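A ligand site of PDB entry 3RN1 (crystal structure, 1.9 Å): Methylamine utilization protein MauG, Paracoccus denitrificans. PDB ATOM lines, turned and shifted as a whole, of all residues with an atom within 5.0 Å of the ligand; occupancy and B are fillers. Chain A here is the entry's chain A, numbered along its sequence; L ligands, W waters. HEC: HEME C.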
ATOM      1  N   PHE A  18     -19.433  29.269  10.076  1.00  0.00           N
ATOM      2  CA  PHE A  18     -18.508  28.399  10.671  1.00  0.00           C
ATOM      3  C   PHE A  18     -17.219  29.132  11.137  1.00  0.00           C
ATOM      4  O   PHE A  18     -16.580  28.705  12.105  1.00  0.00           O
ATOM      5  CB  PHE A  18     -18.133  27.323   9.603  1.00  0.00           C
ATOM      6  CG  PHE A  18     -17.333  26.197  10.168  1.00  0.00           C
ATOM      7  CD1 PHE A  18     -17.982  25.175  10.880  1.00  0.00           C
ATOM      8  CD2 PHE A  18     -15.909  26.175  10.018  1.00  0.00           C
ATOM      9  CE1 PHE A  18     -17.253  24.062  11.397  1.00  0.00           C
ATOM     10  CE2 PHE A  18     -15.182  25.099  10.588  1.00  0.00           C
ATOM     11  CZ  PHE A  18     -15.861  24.072  11.289  1.00  0.00           C
ATOM     12  N   GLN A  29     -14.154  33.415  19.484  1.00  0.00           N
ATOM     13  CA  GLN A  29     -13.999  32.106  18.899  1.00  0.00           C
ATOM     14  C   GLN A  29     -15.147  31.755  18.008  1.00  0.00           C
ATOM     15  O   GLN A  29     -16.247  32.254  18.189  1.00  0.00           O
ATOM     16  CB  GLN A  29     -13.716  31.035  19.979  1.00  0.00           C
ATOM     17  CG  GLN A  29     -14.840  30.621  20.779  1.00  0.00           C
ATOM     18  CD  GLN A  29     -14.439  29.425  21.701  1.00  0.00           C
ATOM     19  OE1 GLN A  29     -13.231  29.101  21.940  1.00  0.00           O
ATOM     20  NE2 GLN A  29     -15.423  28.854  22.269  1.00  0.00           N
ATOM     21  N   SER A  30     -14.848  30.977  17.006  1.00  0.00           N
ATOM     22  CA  SER A  30     -15.807  30.488  16.004  1.00  0.00           C
ATOM     23  C   SER A  30     -15.773  28.938  16.063  1.00  0.00           C
ATOM     24  O   SER A  30     -14.946  28.389  16.800  1.00  0.00           O
ATOM     25  CB  SER A  30     -15.356  30.980  14.612  1.00  0.00           C
ATOM     26  OG  SER A  30     -14.135  30.308  14.214  1.00  0.00           O
ATOM     27  N   CYS A  31     -16.712  28.228  15.399  1.00  0.00           N
ATOM     28  CA  CYS A  31     -16.550  26.749  15.253  1.00  0.00           C
ATOM     29  C   CYS A  31     -15.115  26.370  14.855  1.00  0.00           C
ATOM     30  O   CYS A  31     -14.556  25.418  15.415  1.00  0.00           O
ATOM     31  CB  CYS A  31     -17.483  26.149  14.191  1.00  0.00           C
ATOM     32  SG  CYS A  31     -19.218  26.735  14.289  1.00  0.00           S
ATOM     33  N   CYS A  34     -12.048  25.694  17.445  1.00  0.00           N
ATOM     34  CA  CYS A  34     -11.840  24.399  18.006  1.00  0.00           C
ATOM     35  C   CYS A  34     -11.825  23.309  16.956  1.00  0.00           C
ATOM     36  O   CYS A  34     -11.228  22.258  17.180  1.00  0.00           O
ATOM     37  CB  CYS A  34     -12.959  24.057  18.972  1.00  0.00           C
ATOM     38  SG  CYS A  34     -12.976  25.142  20.421  1.00  0.00           S
ATOM     39  N   HIS A  35     -12.490  23.504  15.848  1.00  0.00           N
ATOM     40  CA  HIS A  35     -12.440  22.502  14.772  1.00  0.00           C
ATOM     41  C   HIS A  35     -11.653  23.069  13.637  1.00  0.00           C
ATOM     42  O   HIS A  35     -12.232  23.494  12.619  1.00  0.00           O
ATOM     43  CB  HIS A  35     -13.871  22.174  14.317  1.00  0.00           C
ATOM     44  CG  HIS A  35     -14.716  21.576  15.397  1.00  0.00           C
ATOM     45  ND1 HIS A  35     -14.635  20.250  15.735  1.00  0.00           N
ATOM     46  CD2 HIS A  35     -15.681  22.109  16.187  1.00  0.00           C
ATOM     47  CE1 HIS A  35     -15.488  19.988  16.715  1.00  0.00           C
ATOM     48  NE2 HIS A  35     -16.171  21.102  16.991  1.00  0.00           N
ATOM     49  N   ARG A  45      -4.805  23.750  19.954  1.00  0.00           N
ATOM     50  CA  ARG A  45      -4.319  24.640  20.982  1.00  0.00           C
ATOM     51  C   ARG A  45      -3.954  23.882  22.252  1.00  0.00           C
ATOM     52  O   ARG A  45      -4.687  22.963  22.627  1.00  0.00           O
ATOM     53  CB  ARG A  45      -5.369  25.693  21.258  1.00  0.00           C
ATOM     54  CG  ARG A  45      -5.586  26.666  20.052  1.00  0.00           C
ATOM     55  CD  ARG A  45      -6.801  27.622  20.312  1.00  0.00           C
ATOM     56  NE  ARG A  45      -8.042  26.837  20.563  1.00  0.00           N
ATOM     57  CZ  ARG A  45      -9.039  27.222  21.355  1.00  0.00           C
ATOM     58  NH1 ARG A  45      -9.007  28.404  21.971  1.00  0.00           N
ATOM     59  NH2 ARG A  45     -10.078  26.434  21.527  1.00  0.00           N
ATOM     60  N   SER A  54     -10.645  21.407  25.137  1.00  0.00           N
ATOM     61  CA  SER A  54     -10.513  22.732  24.480  1.00  0.00           C
ATOM     62  C   SER A  54     -10.939  23.831  25.456  1.00  0.00           C
ATOM     63  O   SER A  54     -11.752  23.593  26.335  1.00  0.00           O
ATOM     64  CB  SER A  54     -11.449  22.750  23.284  1.00  0.00           C
ATOM     65  OG  SER A  54     -10.919  21.962  22.206  1.00  0.00           O
ATOM     66  N   VAL A  55     -10.372  25.020  25.278  1.00  0.00           N
ATOM     67  CA  VAL A  55     -10.742  26.206  26.083  1.00  0.00           C
ATOM     68  C   VAL A  55     -11.853  27.001  25.412  1.00  0.00           C
ATOM     69  O   VAL A  55     -11.808  27.204  24.171  1.00  0.00           O
ATOM     70  CB  VAL A  55      -9.540  27.094  26.249  1.00  0.00           C
ATOM     71  CG1 VAL A  55      -9.922  28.316  27.106  1.00  0.00           C
ATOM     72  CG2 VAL A  55      -8.407  26.281  26.926  1.00  0.00           C
ATOM     73  N   GLY A  56     -12.797  27.503  26.201  1.00  0.00           N
ATOM     74  CA  GLY A  56     -14.005  28.230  25.632  1.00  0.00           C
ATOM     75  C   GLY A  56     -13.723  29.702  25.331  1.00  0.00           C
ATOM     76  O   GLY A  56     -12.620  30.192  25.584  1.00  0.00           O
ATOM     77  N   ARG A  65     -14.414  16.820  27.614  1.00  0.00           N
ATOM     78  CA  ARG A  65     -14.213  15.825  26.570  1.00  0.00           C
ATOM     79  C   ARG A  65     -13.367  16.401  25.455  1.00  0.00           C
ATOM     80  O   ARG A  65     -13.363  17.614  25.278  1.00  0.00           O
ATOM     81  CB  ARG A  65     -15.549  15.388  26.014  1.00  0.00           C
ATOM     82  CG  ARG A  65     -16.406  14.657  27.103  1.00  0.00           C
ATOM     83  CD  ARG A  65     -17.627  14.152  26.445  1.00  0.00           C
ATOM     84  NE  ARG A  65     -18.450  13.371  27.361  1.00  0.00           N
ATOM     85  CZ  ARG A  65     -19.775  13.258  27.220  1.00  0.00           C
ATOM     86  NH1 ARG A  65     -20.375  13.891  26.233  1.00  0.00           N
ATOM     87  NH2 ARG A  65     -20.491  12.516  28.075  1.00  0.00           N
ATOM     88  N   ASN A  66     -12.714  15.524  24.688  1.00  0.00           N
ATOM     89  CA  ASN A  66     -11.819  15.925  23.606  1.00  0.00           C
ATOM     90  C   ASN A  66     -12.639  16.397  22.370  1.00  0.00           C
ATOM     91  O   ASN A  66     -13.665  15.778  21.990  1.00  0.00           O
ATOM     92  CB  ASN A  66     -10.998  14.689  23.181  1.00  0.00           C
ATOM     93  CG  ASN A  66      -9.949  15.027  22.141  1.00  0.00           C
ATOM     94  OD1 ASN A  66      -9.025  15.883  22.353  1.00  0.00           O
ATOM     95  ND2 ASN A  66     -10.089  14.416  21.006  1.00  0.00           N
ATOM     96  N   THR A  67     -12.183  17.467  21.745  1.00  0.00           N
ATOM     97  CA  THR A  67     -12.912  17.921  20.537  1.00  0.00           C
ATOM     98  C   THR A  67     -12.742  16.939  19.332  1.00  0.00           C
ATOM     99  O   THR A  67     -11.677  16.734  18.884  1.00  0.00           O
ATOM    100  CB  THR A  67     -12.437  19.337  20.153  1.00  0.00           C
ATOM    101  OG1 THR A  67     -12.713  20.253  21.229  1.00  0.00           O
ATOM    102  CG2 THR A  67     -13.056  19.806  18.839  1.00  0.00           C
ATOM    103  N   PRO A  68     -13.828  16.342  18.829  1.00  0.00           N
ATOM    104  CA  PRO A  68     -13.750  15.390  17.739  1.00  0.00           C
ATOM    105  C   PRO A  68     -13.592  16.119  16.385  1.00  0.00           C
ATOM    106  O   PRO A  68     -13.995  17.274  16.195  1.00  0.00           O
ATOM    107  CB  PRO A  68     -15.112  14.654  17.794  1.00  0.00           C
ATOM    108  CG  PRO A  68     -16.003  15.694  18.277  1.00  0.00           C
ATOM    109  CD  PRO A  68     -15.222  16.503  19.294  1.00  0.00           C
ATOM    110  N   THR A  69     -13.076  15.399  15.401  1.00  0.00           N
ATOM    111  CA  THR A  69     -13.154  15.853  14.009  1.00  0.00           C
ATOM    112  C   THR A  69     -14.583  16.034  13.506  1.00  0.00           C
ATOM    113  O   THR A  69     -15.507  15.306  13.892  1.00  0.00           O
ATOM    114  CB  THR A  69     -12.403  14.868  13.038  1.00  0.00           C
ATOM    115  OG1 THR A  69     -12.390  15.492  11.743  1.00  0.00           O
ATOM    116  CG2 THR A  69     -13.057  13.452  12.968  1.00  0.00           C
ATOM    117  N   LEU A  70     -14.769  16.959  12.586  1.00  0.00           N
ATOM    118  CA  LEU A  70     -16.051  17.031  11.941  1.00  0.00           C
ATOM    119  C   LEU A  70     -16.015  16.341  10.583  1.00  0.00           C
ATOM    120  O   LEU A  70     -17.049  16.259   9.905  1.00  0.00           O
ATOM    121  CB  LEU A  70     -16.451  18.514  11.726  1.00  0.00           C
ATOM    122  CG  LEU A  70     -16.517  19.408  13.002  1.00  0.00           C
ATOM    123  CD1 LEU A  70     -16.963  20.821  12.598  1.00  0.00           C
ATOM    124  CD2 LEU A  70     -17.441  18.803  13.999  1.00  0.00           C
ATOM    125  N   ALA A  73     -18.615  13.418   9.744  1.00  0.00           N
ATOM    126  CA  ALA A  73     -19.660  13.366  10.760  1.00  0.00           C
ATOM    127  C   ALA A  73     -21.017  13.359  10.074  1.00  0.00           C
ATOM    128  O   ALA A  73     -22.005  12.858  10.631  1.00  0.00           O
ATOM    129  CB  ALA A  73     -19.528  14.518  11.743  1.00  0.00           C
ATOM    130  N   GLN A  91     -24.995  12.626  17.592  1.00  0.00           N
ATOM    131  CA  GLN A  91     -23.759  13.453  17.652  1.00  0.00           C
ATOM    132  C   GLN A  91     -23.423  13.752  19.105  1.00  0.00           C
ATOM    133  O   GLN A  91     -24.283  13.652  19.962  1.00  0.00           O
ATOM    134  CB  GLN A  91     -23.895  14.752  16.820  1.00  0.00           C
ATOM    135  CG  GLN A  91     -24.303  14.479  15.326  1.00  0.00           C
ATOM    136  CD  GLN A  91     -23.129  13.976  14.427  1.00  0.00           C
ATOM    137  OE1 GLN A  91     -23.361  13.403  13.331  1.00  0.00           O
ATOM    138  NE2 GLN A  91     -21.933  14.229  14.848  1.00  0.00           N
ATOM    139  N   PHE A  92     -22.154  14.155  19.315  1.00  0.00           N
ATOM    140  CA  PHE A  92     -21.452  14.185  20.574  1.00  0.00           C
ATOM    141  C   PHE A  92     -20.985  12.751  20.974  1.00  0.00           C
ATOM    142  O   PHE A  92     -21.548  11.748  20.522  1.00  0.00           O
ATOM    143  CB  PHE A  92     -22.262  14.783  21.693  1.00  0.00           C
ATOM    144  CG  PHE A  92     -22.502  16.257  21.558  1.00  0.00           C
ATOM    145  CD1 PHE A  92     -21.439  17.171  21.452  1.00  0.00           C
ATOM    146  CD2 PHE A  92     -23.821  16.748  21.579  1.00  0.00           C
ATOM    147  CE1 PHE A  92     -21.675  18.552  21.428  1.00  0.00           C
ATOM    148  CE2 PHE A  92     -24.057  18.146  21.540  1.00  0.00           C
ATOM    149  CZ  PHE A  92     -22.963  19.029  21.466  1.00  0.00           C
ATOM    150  N   TRP A  93     -19.964  12.675  21.824  1.00  0.00           N
ATOM    151  CA  TRP A  93     -19.424  11.375  22.237  1.00  0.00           C
ATOM    152  C   TRP A  93     -20.497  10.584  22.995  1.00  0.00           C
ATOM    153  O   TRP A  93     -20.401   9.374  23.058  1.00  0.00           O
ATOM    154  CB  TRP A  93     -18.208  11.567  23.146  1.00  0.00           C
ATOM    155  CG  TRP A  93     -16.929  12.049  22.507  1.00  0.00           C
ATOM    156  CD1 TRP A  93     -16.458  13.329  22.509  1.00  0.00           C
ATOM    157  CD2 TRP A  93     -15.909  11.229  21.899  1.00  0.00           C
ATOM    158  NE1 TRP A  93     -15.226  13.379  21.904  1.00  0.00           N
ATOM    159  CE2 TRP A  93     -14.864  12.125  21.496  1.00  0.00           C
ATOM    160  CE3 TRP A  93     -15.782   9.849  21.638  1.00  0.00           C
ATOM    161  CZ2 TRP A  93     -13.684  11.672  20.864  1.00  0.00           C
ATOM    162  CZ3 TRP A  93     -14.571   9.370  21.015  1.00  0.00           C
ATOM    163  CH2 TRP A  93     -13.547  10.289  20.625  1.00  0.00           C
ATOM    164  N   ASP A  94     -21.479  11.254  23.618  1.00  0.00           N
ATOM    165  CA  ASP A  94     -22.585  10.546  24.308  1.00  0.00           C
ATOM    166  C   ASP A  94     -23.900  10.493  23.532  1.00  0.00           C
ATOM    167  O   ASP A  94     -24.963  10.096  24.067  1.00  0.00           O
ATOM    168  CB  ASP A  94     -22.855  11.125  25.684  1.00  0.00           C
ATOM    169  CG  ASP A  94     -23.137  12.632  25.632  1.00  0.00           C
ATOM    170  OD1 ASP A  94     -23.107  13.242  26.713  1.00  0.00           O
ATOM    171  OD2 ASP A  94     -23.352  13.191  24.508  1.00  0.00           O
ATOM    172  N   ARG A  96     -25.931  12.742  22.644  1.00  0.00           N
ATOM    173  CA  ARG A  96     -27.017  13.497  23.187  1.00  0.00           C
ATOM    174  C   ARG A  96     -27.730  14.364  22.200  1.00  0.00           C
ATOM    175  O   ARG A  96     -28.845  14.774  22.470  1.00  0.00           O
ATOM    176  CB  ARG A  96     -26.637  14.290  24.429  1.00  0.00           C
ATOM    177  CG  ARG A  96     -25.747  15.444  24.144  1.00  0.00           C
ATOM    178  CD  ARG A  96     -25.360  16.104  25.499  1.00  0.00           C
ATOM    179  NE  ARG A  96     -24.479  17.244  25.312  1.00  0.00           N
ATOM    180  CZ  ARG A  96     -23.171  17.149  25.149  1.00  0.00           C
ATOM    181  NH1 ARG A  96     -22.399  18.234  25.039  1.00  0.00           N
ATOM    182  NH2 ARG A  96     -22.635  15.944  25.117  1.00  0.00           N
ATOM    183  N   LEU A 100     -26.867  16.550  13.111  1.00  0.00           N
ATOM    184  CA  LEU A 100     -25.981  17.751  13.052  1.00  0.00           C
ATOM    185  C   LEU A 100     -26.745  19.056  13.248  1.00  0.00           C
ATOM    186  O   LEU A 100     -26.230  20.024  13.835  1.00  0.00           O
ATOM    187  CB  LEU A 100     -25.285  17.793  11.686  1.00  0.00           C
ATOM    188  CG  LEU A 100     -24.167  16.797  11.446  1.00  0.00           C
ATOM    189  CD1 LEU A 100     -23.789  16.812   9.904  1.00  0.00           C
ATOM    190  CD2 LEU A 100     -23.003  17.200  12.333  1.00  0.00           C
ATOM    191  N   GLN A 103     -27.316  19.427  16.863  1.00  0.00           N
ATOM    192  CA  GLN A 103     -26.061  19.662  17.593  1.00  0.00           C
ATOM    193  C   GLN A 103     -25.590  21.125  17.508  1.00  0.00           C
ATOM    194  O   GLN A 103     -25.054  21.665  18.475  1.00  0.00           O
ATOM    195  CB  GLN A 103     -24.998  18.783  17.024  1.00  0.00           C
ATOM    196  CG  GLN A 103     -23.709  18.760  17.832  1.00  0.00           C
ATOM    197  CD  GLN A 103     -22.824  19.996  17.543  1.00  0.00           C
ATOM    198  OE1 GLN A 103     -22.935  20.664  16.483  1.00  0.00           O
ATOM    199  NE2 GLN A 103     -21.935  20.309  18.492  1.00  0.00           N
ATOM    200  N   ALA A 104     -25.779  21.772  16.359  1.00  0.00           N
ATOM    201  CA  ALA A 104     -24.983  23.013  16.034  1.00  0.00           C
ATOM    202  C   ALA A 104     -25.233  24.189  16.991  1.00  0.00           C
ATOM    203  O   ALA A 104     -24.339  25.019  17.262  1.00  0.00           O
ATOM    204  CB  ALA A 104     -25.241  23.472  14.585  1.00  0.00           C
ATOM    205  N   PRO A 107     -22.966  24.258  21.083  1.00  0.00           N
ATOM    206  CA  PRO A 107     -21.718  25.009  21.480  1.00  0.00           C
ATOM    207  C   PRO A 107     -21.991  26.511  21.618  1.00  0.00           C
ATOM    208  O   PRO A 107     -21.362  27.201  22.479  1.00  0.00           O
ATOM    209  CB  PRO A 107     -20.749  24.805  20.289  1.00  0.00           C
ATOM    210  CG  PRO A 107     -21.291  23.646  19.455  1.00  0.00           C
ATOM    211  CD  PRO A 107     -22.831  23.558  19.782  1.00  0.00           C
ATOM    212  N   MET A 108     -22.897  27.043  20.769  1.00  0.00           N
ATOM    213  CA  MET A 108     -23.205  28.469  20.835  1.00  0.00           C
ATOM    214  C   MET A 108     -23.650  28.947  22.217  1.00  0.00           C
ATOM    215  O   MET A 108     -23.272  30.052  22.624  1.00  0.00           O
ATOM    216  CB  MET A 108     -24.255  28.900  19.815  1.00  0.00           C
ATOM    217  CG  MET A 108     -23.809  28.777  18.358  1.00  0.00           C
ATOM    218  SD  MET A 108     -25.180  29.235  17.240  1.00  0.00           S
ATOM    219  CE  MET A 108     -24.788  28.250  15.779  1.00  0.00           C
ATOM    220  N   VAL A 112     -19.269  26.925  28.781  1.00  0.00           N
ATOM    221  CA  VAL A 112     -17.844  26.501  28.721  1.00  0.00           C
ATOM    222  C   VAL A 112     -17.286  26.516  27.287  1.00  0.00           C
ATOM    223  O   VAL A 112     -16.067  26.405  27.086  1.00  0.00           O
ATOM    224  CB  VAL A 112     -17.506  25.189  29.582  1.00  0.00           C
ATOM    225  CG1 VAL A 112     -18.530  24.939  30.700  1.00  0.00           C
ATOM    226  CG2 VAL A 112     -17.246  23.981  28.792  1.00  0.00           C
ATOM    227  N   GLU A 113     -18.165  26.772  26.313  1.00  0.00           N
ATOM    228  CA  GLU A 113     -17.718  26.969  24.948  1.00  0.00           C
ATOM    229  C   GLU A 113     -17.955  28.414  24.476  1.00  0.00           C
ATOM    230  O   GLU A 113     -17.318  29.349  25.003  1.00  0.00           O
ATOM    231  CB  GLU A 113     -18.294  25.877  24.031  1.00  0.00           C
ATOM    232  CG  GLU A 113     -17.890  24.459  24.634  1.00  0.00           C
ATOM    233  CD  GLU A 113     -18.521  23.261  23.894  1.00  0.00           C
ATOM    234  OE1 GLU A 113     -19.678  23.393  23.494  1.00  0.00           O
ATOM    235  OE2 GLU A 113     -17.889  22.157  23.801  1.00  0.00           O
ATOM    236  N   MET A 114     -18.860  28.595  23.504  1.00  0.00           N
ATOM    237  CA  MET A 114     -18.989  29.919  22.852  1.00  0.00           C
ATOM    238  C   MET A 114     -19.738  30.887  23.766  1.00  0.00           C
ATOM    239  O   MET A 114     -19.623  32.096  23.593  1.00  0.00           O
ATOM    240  CB  MET A 114     -19.685  29.774  21.491  1.00  0.00           C
ATOM    241  CG  MET A 114     -18.818  28.844  20.578  1.00  0.00           C
ATOM    242  SD  MET A 114     -19.571  28.501  18.952  1.00  0.00           S
ATOM    243  CE  MET A 114     -18.868  29.842  18.073  1.00  0.00           C
ATOM    244  N   LEU A 159     -25.252  25.518   9.102  1.00  0.00           N
ATOM    245  CA  LEU A 159     -24.021  24.931   9.608  1.00  0.00           C
ATOM    246  C   LEU A 159     -24.037  23.414   9.333  1.00  0.00           C
ATOM    247  O   LEU A 159     -23.064  22.881   8.920  1.00  0.00           O
ATOM    248  CB  LEU A 159     -23.915  25.220  11.101  1.00  0.00           C
ATOM    249  CG  LEU A 159     -23.310  26.567  11.472  1.00  0.00           C
ATOM    250  CD1 LEU A 159     -23.570  26.788  12.977  1.00  0.00           C
ATOM    251  CD2 LEU A 159     -21.799  26.820  11.178  1.00  0.00           C
ATOM    252  N   GLN A 163     -21.510  21.240   6.815  1.00  0.00           N
ATOM    253  CA  GLN A 163     -20.775  20.029   7.248  1.00  0.00           C
ATOM    254  C   GLN A 163     -21.114  18.806   6.376  1.00  0.00           C
ATOM    255  O   GLN A 163     -20.360  17.830   6.373  1.00  0.00           O
ATOM    256  CB  GLN A 163     -21.066  19.691   8.743  1.00  0.00           C
ATOM    257  CG  GLN A 163     -20.395  20.694   9.730  1.00  0.00           C
ATOM    258  CD  GLN A 163     -20.932  20.476  11.111  1.00  0.00           C
ATOM    259  OE1 GLN A 163     -20.429  19.639  11.854  1.00  0.00           O
ATOM    260  NE2 GLN A 163     -21.946  21.221  11.470  1.00  0.00           N
ATOM    261  N   LYS A 265     -19.865   6.828  21.841  1.00  0.00           N
ATOM    262  CA  LYS A 265     -19.952   6.558  20.374  1.00  0.00           C
ATOM    263  C   LYS A 265     -18.633   6.125  19.781  1.00  0.00           C
ATOM    264  O   LYS A 265     -17.566   6.723  20.085  1.00  0.00           O
ATOM    265  CB  LYS A 265     -20.575   7.768  19.641  1.00  0.00           C
ATOM    266  CG  LYS A 265     -20.769   7.621  18.114  1.00  0.00           C
ATOM    267  CD  LYS A 265     -21.516   8.894  17.506  1.00  0.00           C
ATOM    268  CE  LYS A 265     -20.748  10.216  17.731  1.00  0.00           C
ATOM    269  NZ  LYS A 265     -19.421  10.385  17.020  1.00  0.00           N
HETATM  270 FE   HEC L   1     -17.875  21.355  18.371  1.00  0.00          FE
HETATM  271  CHA HEC L   1     -18.504  18.112  19.207  1.00  0.00           C
HETATM  272  CHB HEC L   1     -19.827  21.062  15.596  1.00  0.00           C
HETATM  273  CHC HEC L   1     -18.010  24.763  18.043  1.00  0.00           C
HETATM  274  CHD HEC L   1     -15.559  21.602  20.928  1.00  0.00           C
HETATM  275  NA  HEC L   1     -18.916  19.791  17.461  1.00  0.00           N
HETATM  276  C1A HEC L   1     -19.113  18.568  17.950  1.00  0.00           C
HETATM  277  C2A HEC L   1     -19.798  17.646  16.990  1.00  0.00           C
HETATM  278  C3A HEC L   1     -20.259  18.490  15.984  1.00  0.00           C
HETATM  279  C4A HEC L   1     -19.684  19.828  16.367  1.00  0.00           C
HETATM  280  CMA HEC L   1     -21.041  18.087  14.720  1.00  0.00           C
HETATM  281  CAA HEC L   1     -20.060  16.181  17.206  1.00  0.00           C
HETATM  282  CBA HEC L   1     -19.099  15.350  16.432  1.00  0.00           C
HETATM  283  CGA HEC L   1     -19.140  13.865  16.857  1.00  0.00           C
HETATM  284  O1A HEC L   1     -18.500  13.039  16.190  1.00  0.00           O
HETATM  285  O2A HEC L   1     -19.765  13.473  17.849  1.00  0.00           O
HETATM  286  NB  HEC L   1     -18.721  22.679  17.014  1.00  0.00           N
HETATM  287  C1B HEC L   1     -19.573  22.420  16.029  1.00  0.00           C
HETATM  288  C2B HEC L   1     -20.135  23.619  15.353  1.00  0.00           C
HETATM  289  C3B HEC L   1     -19.598  24.705  16.051  1.00  0.00           C
HETATM  290  C4B HEC L   1     -18.805  24.018  17.100  1.00  0.00           C
HETATM  291  CMB HEC L   1     -21.057  23.559  14.139  1.00  0.00           C
HETATM  292  CAB HEC L   1     -19.830  26.218  15.904  1.00  0.00           C
HETATM  293  CBB HEC L   1     -21.270  26.498  16.290  1.00  0.00           C
HETATM  294  NC  HEC L   1     -16.904  22.908  19.325  1.00  0.00           N
HETATM  295  C1C HEC L   1     -17.103  24.200  19.068  1.00  0.00           C
HETATM  296  C2C HEC L   1     -16.163  25.067  19.799  1.00  0.00           C
HETATM  297  C3C HEC L   1     -15.449  24.189  20.611  1.00  0.00           C
HETATM  298  C4C HEC L   1     -16.016  22.868  20.317  1.00  0.00           C
HETATM  299  CMC HEC L   1     -16.054  26.570  19.631  1.00  0.00           C
HETATM  300  CAC HEC L   1     -14.314  24.401  21.596  1.00  0.00           C
HETATM  301  CBC HEC L   1     -14.577  25.425  22.713  1.00  0.00           C
HETATM  302  ND  HEC L   1     -17.090  20.043  19.775  1.00  0.00           N
HETATM  303  C1D HEC L   1     -16.330  20.320  20.837  1.00  0.00           C
HETATM  304  C2D HEC L   1     -16.297  19.243  21.872  1.00  0.00           C
HETATM  305  C3D HEC L   1     -17.163  18.271  21.403  1.00  0.00           C
HETATM  306  C4D HEC L   1     -17.627  18.835  20.096  1.00  0.00           C
HETATM  307  CMD HEC L   1     -15.513  19.243  23.153  1.00  0.00           C
HETATM  308  CAD HEC L   1     -17.525  16.958  22.072  1.00  0.00           C
HETATM  309  CBD HEC L   1     -18.295  17.349  23.327  1.00  0.00           C
HETATM  310  CGD HEC L   1     -19.106  16.186  23.878  1.00  0.00           C
HETATM  311  O1D HEC L   1     -19.813  16.381  24.891  1.00  0.00           O
HETATM  312  O2D HEC L   1     -19.152  15.082  23.280  1.00  0.00           O
HETATM  313  O   HOH W   1     -18.949  17.986  26.589  1.00  0.00           O
HETATM  314  O   HOH W   2     -16.511  12.899  14.584  1.00  0.00           O
HETATM  315  O   HOH W   3     -13.247  20.435  25.455  1.00  0.00           O
HETATM  316  O   HOH W   4     -19.742  12.146  14.144  1.00  0.00           O
HETATM  317  O   HOH W   5     -19.569  21.049  21.601  1.00  0.00           O
HETATM  318  O   HOH W   6     -17.653  12.622  19.165  1.00  0.00           O
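The side-chain sulfur (SG) of Cys 31 is bonded to a carbon (CAB) of the ligand. CAC of the ligand is bonded to SG of Cys 34, at 1.9 Å. A ring nitrogen (NE2) of His 35 binds an iron atom (FE) of the ligand, 2.2 Å away. An oxygen (O1D) of the ligand is in salt-bridge range of the guanidinium group (NH2) of Arg 96 (2.9 Å). O1D of the ligand lies within salt-bridge range of NH1 of Arg 65 (2.9 Å). The backbone NH of Phe 92 is in hydrogen-bond range of an oxygen (O2A) of the ligand (2.9 Å). An oxygen (O2D) of the ligand is in hydrogen-bond range of the backbone NH (N) of Trp 93, at 2.9 Å. An oxygen (O1A) of the ligand lies within salt-bridge range of the side-chain amino group of Lys 265 (2.9 Å).
The backbone carbonyl oxygen (O) of Phe 18 lies within hydrogen-bond range of the backbone NH (N) of Cys 31, at 3.3 Å. A ring nitrogen (ND1) of His 35 is in hydrogen-bond range of the backbone carbonyl oxygen (O) of Pro 68 (3.1 Å). The guanidinium group of Arg 65 is in salt-bridge range of the side-chain carboxylate of Asp 94. OG of Ser 54 sits at hydrogen-bond distance from OG1 of Thr 67 (2.7 Å). The backbone carbonyl oxygen (O) of Ala 73 sits close to the side-chain amide oxygen (OE1) of Gln 91 (3.1 Å). N of Met 114 is in hydrogen-bond range of O of Pro 107, 3.0 Å away. OE1 of Gln 29 lies close to O of Val 55 (3.3 Å). The side-chain amide nitrogen (NE2) of Gln 29 lies within hydrogen-bond range of the backbone carbonyl oxygen (O) of Glu 113 (3.4 Å).
A nitrogen (NA) of the ligand sits close to the side-chain amide nitrogen (NE2) of Gln 103, at 3.2 Å. Residues that only touch the ligand: Gln 29 (3.5 Å), Ser 30 (3.5 Å), Ser 54 (3.7 Å), Val 55 (3.6 Å), Thr 67 (3.2 Å), Pro 68 (3.4 Å), Leu 70 (3.4 Å), Gln 91 (3.4 Å), Leu 100 (3.2 Å), Ala 104 (3.5 Å), Pro 107 (3.4 Å), Met 108 (3.96 Å), Glu 113 (3.7 Å), Met 114 (3.7 Å) and Gln 163 (3.3 Å). Hydrophobic or aromatic side chains within 4 Å of the ligand: His 35, Pro 68, Leu 70, Phe 92, Trp 93, Leu 100, Pro 107, Met 108 and Met 114. Within 4 Å of the ligand: Gln 29, Ser 30, Cys 31, Cys 34, His 35, Ser 54, Val 55, Arg 65, Thr 67, Pro 68, Leu 70, Gln 91, Phe 92, Trp 93, Arg 96, Leu 100, Gln 103, Ala 104, Pro 107, Met 108, Glu 113, Met 114, Gln 163 and Lys 265.
Water W4 lies within hydrogen-bond range of an oxygen (O1A) of the ligand (2.6 Å), the side-chain amide nitrogen (NE2) of Gln 91 (3.1 Å) and the side-chain amino group (NZ) of Lys 265 (3.4 Å). Water W2 lies within hydrogen-bond range of O1A of the ligand (2.6 Å) and O of Thr 69 (2.7 Å). Water W3 lies within hydrogen-bond range of the backbone NH (N) of Ser 54 (2.8 Å) and the backbone carbonyl oxygen (O) of Arg 65 (2.8 Å).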
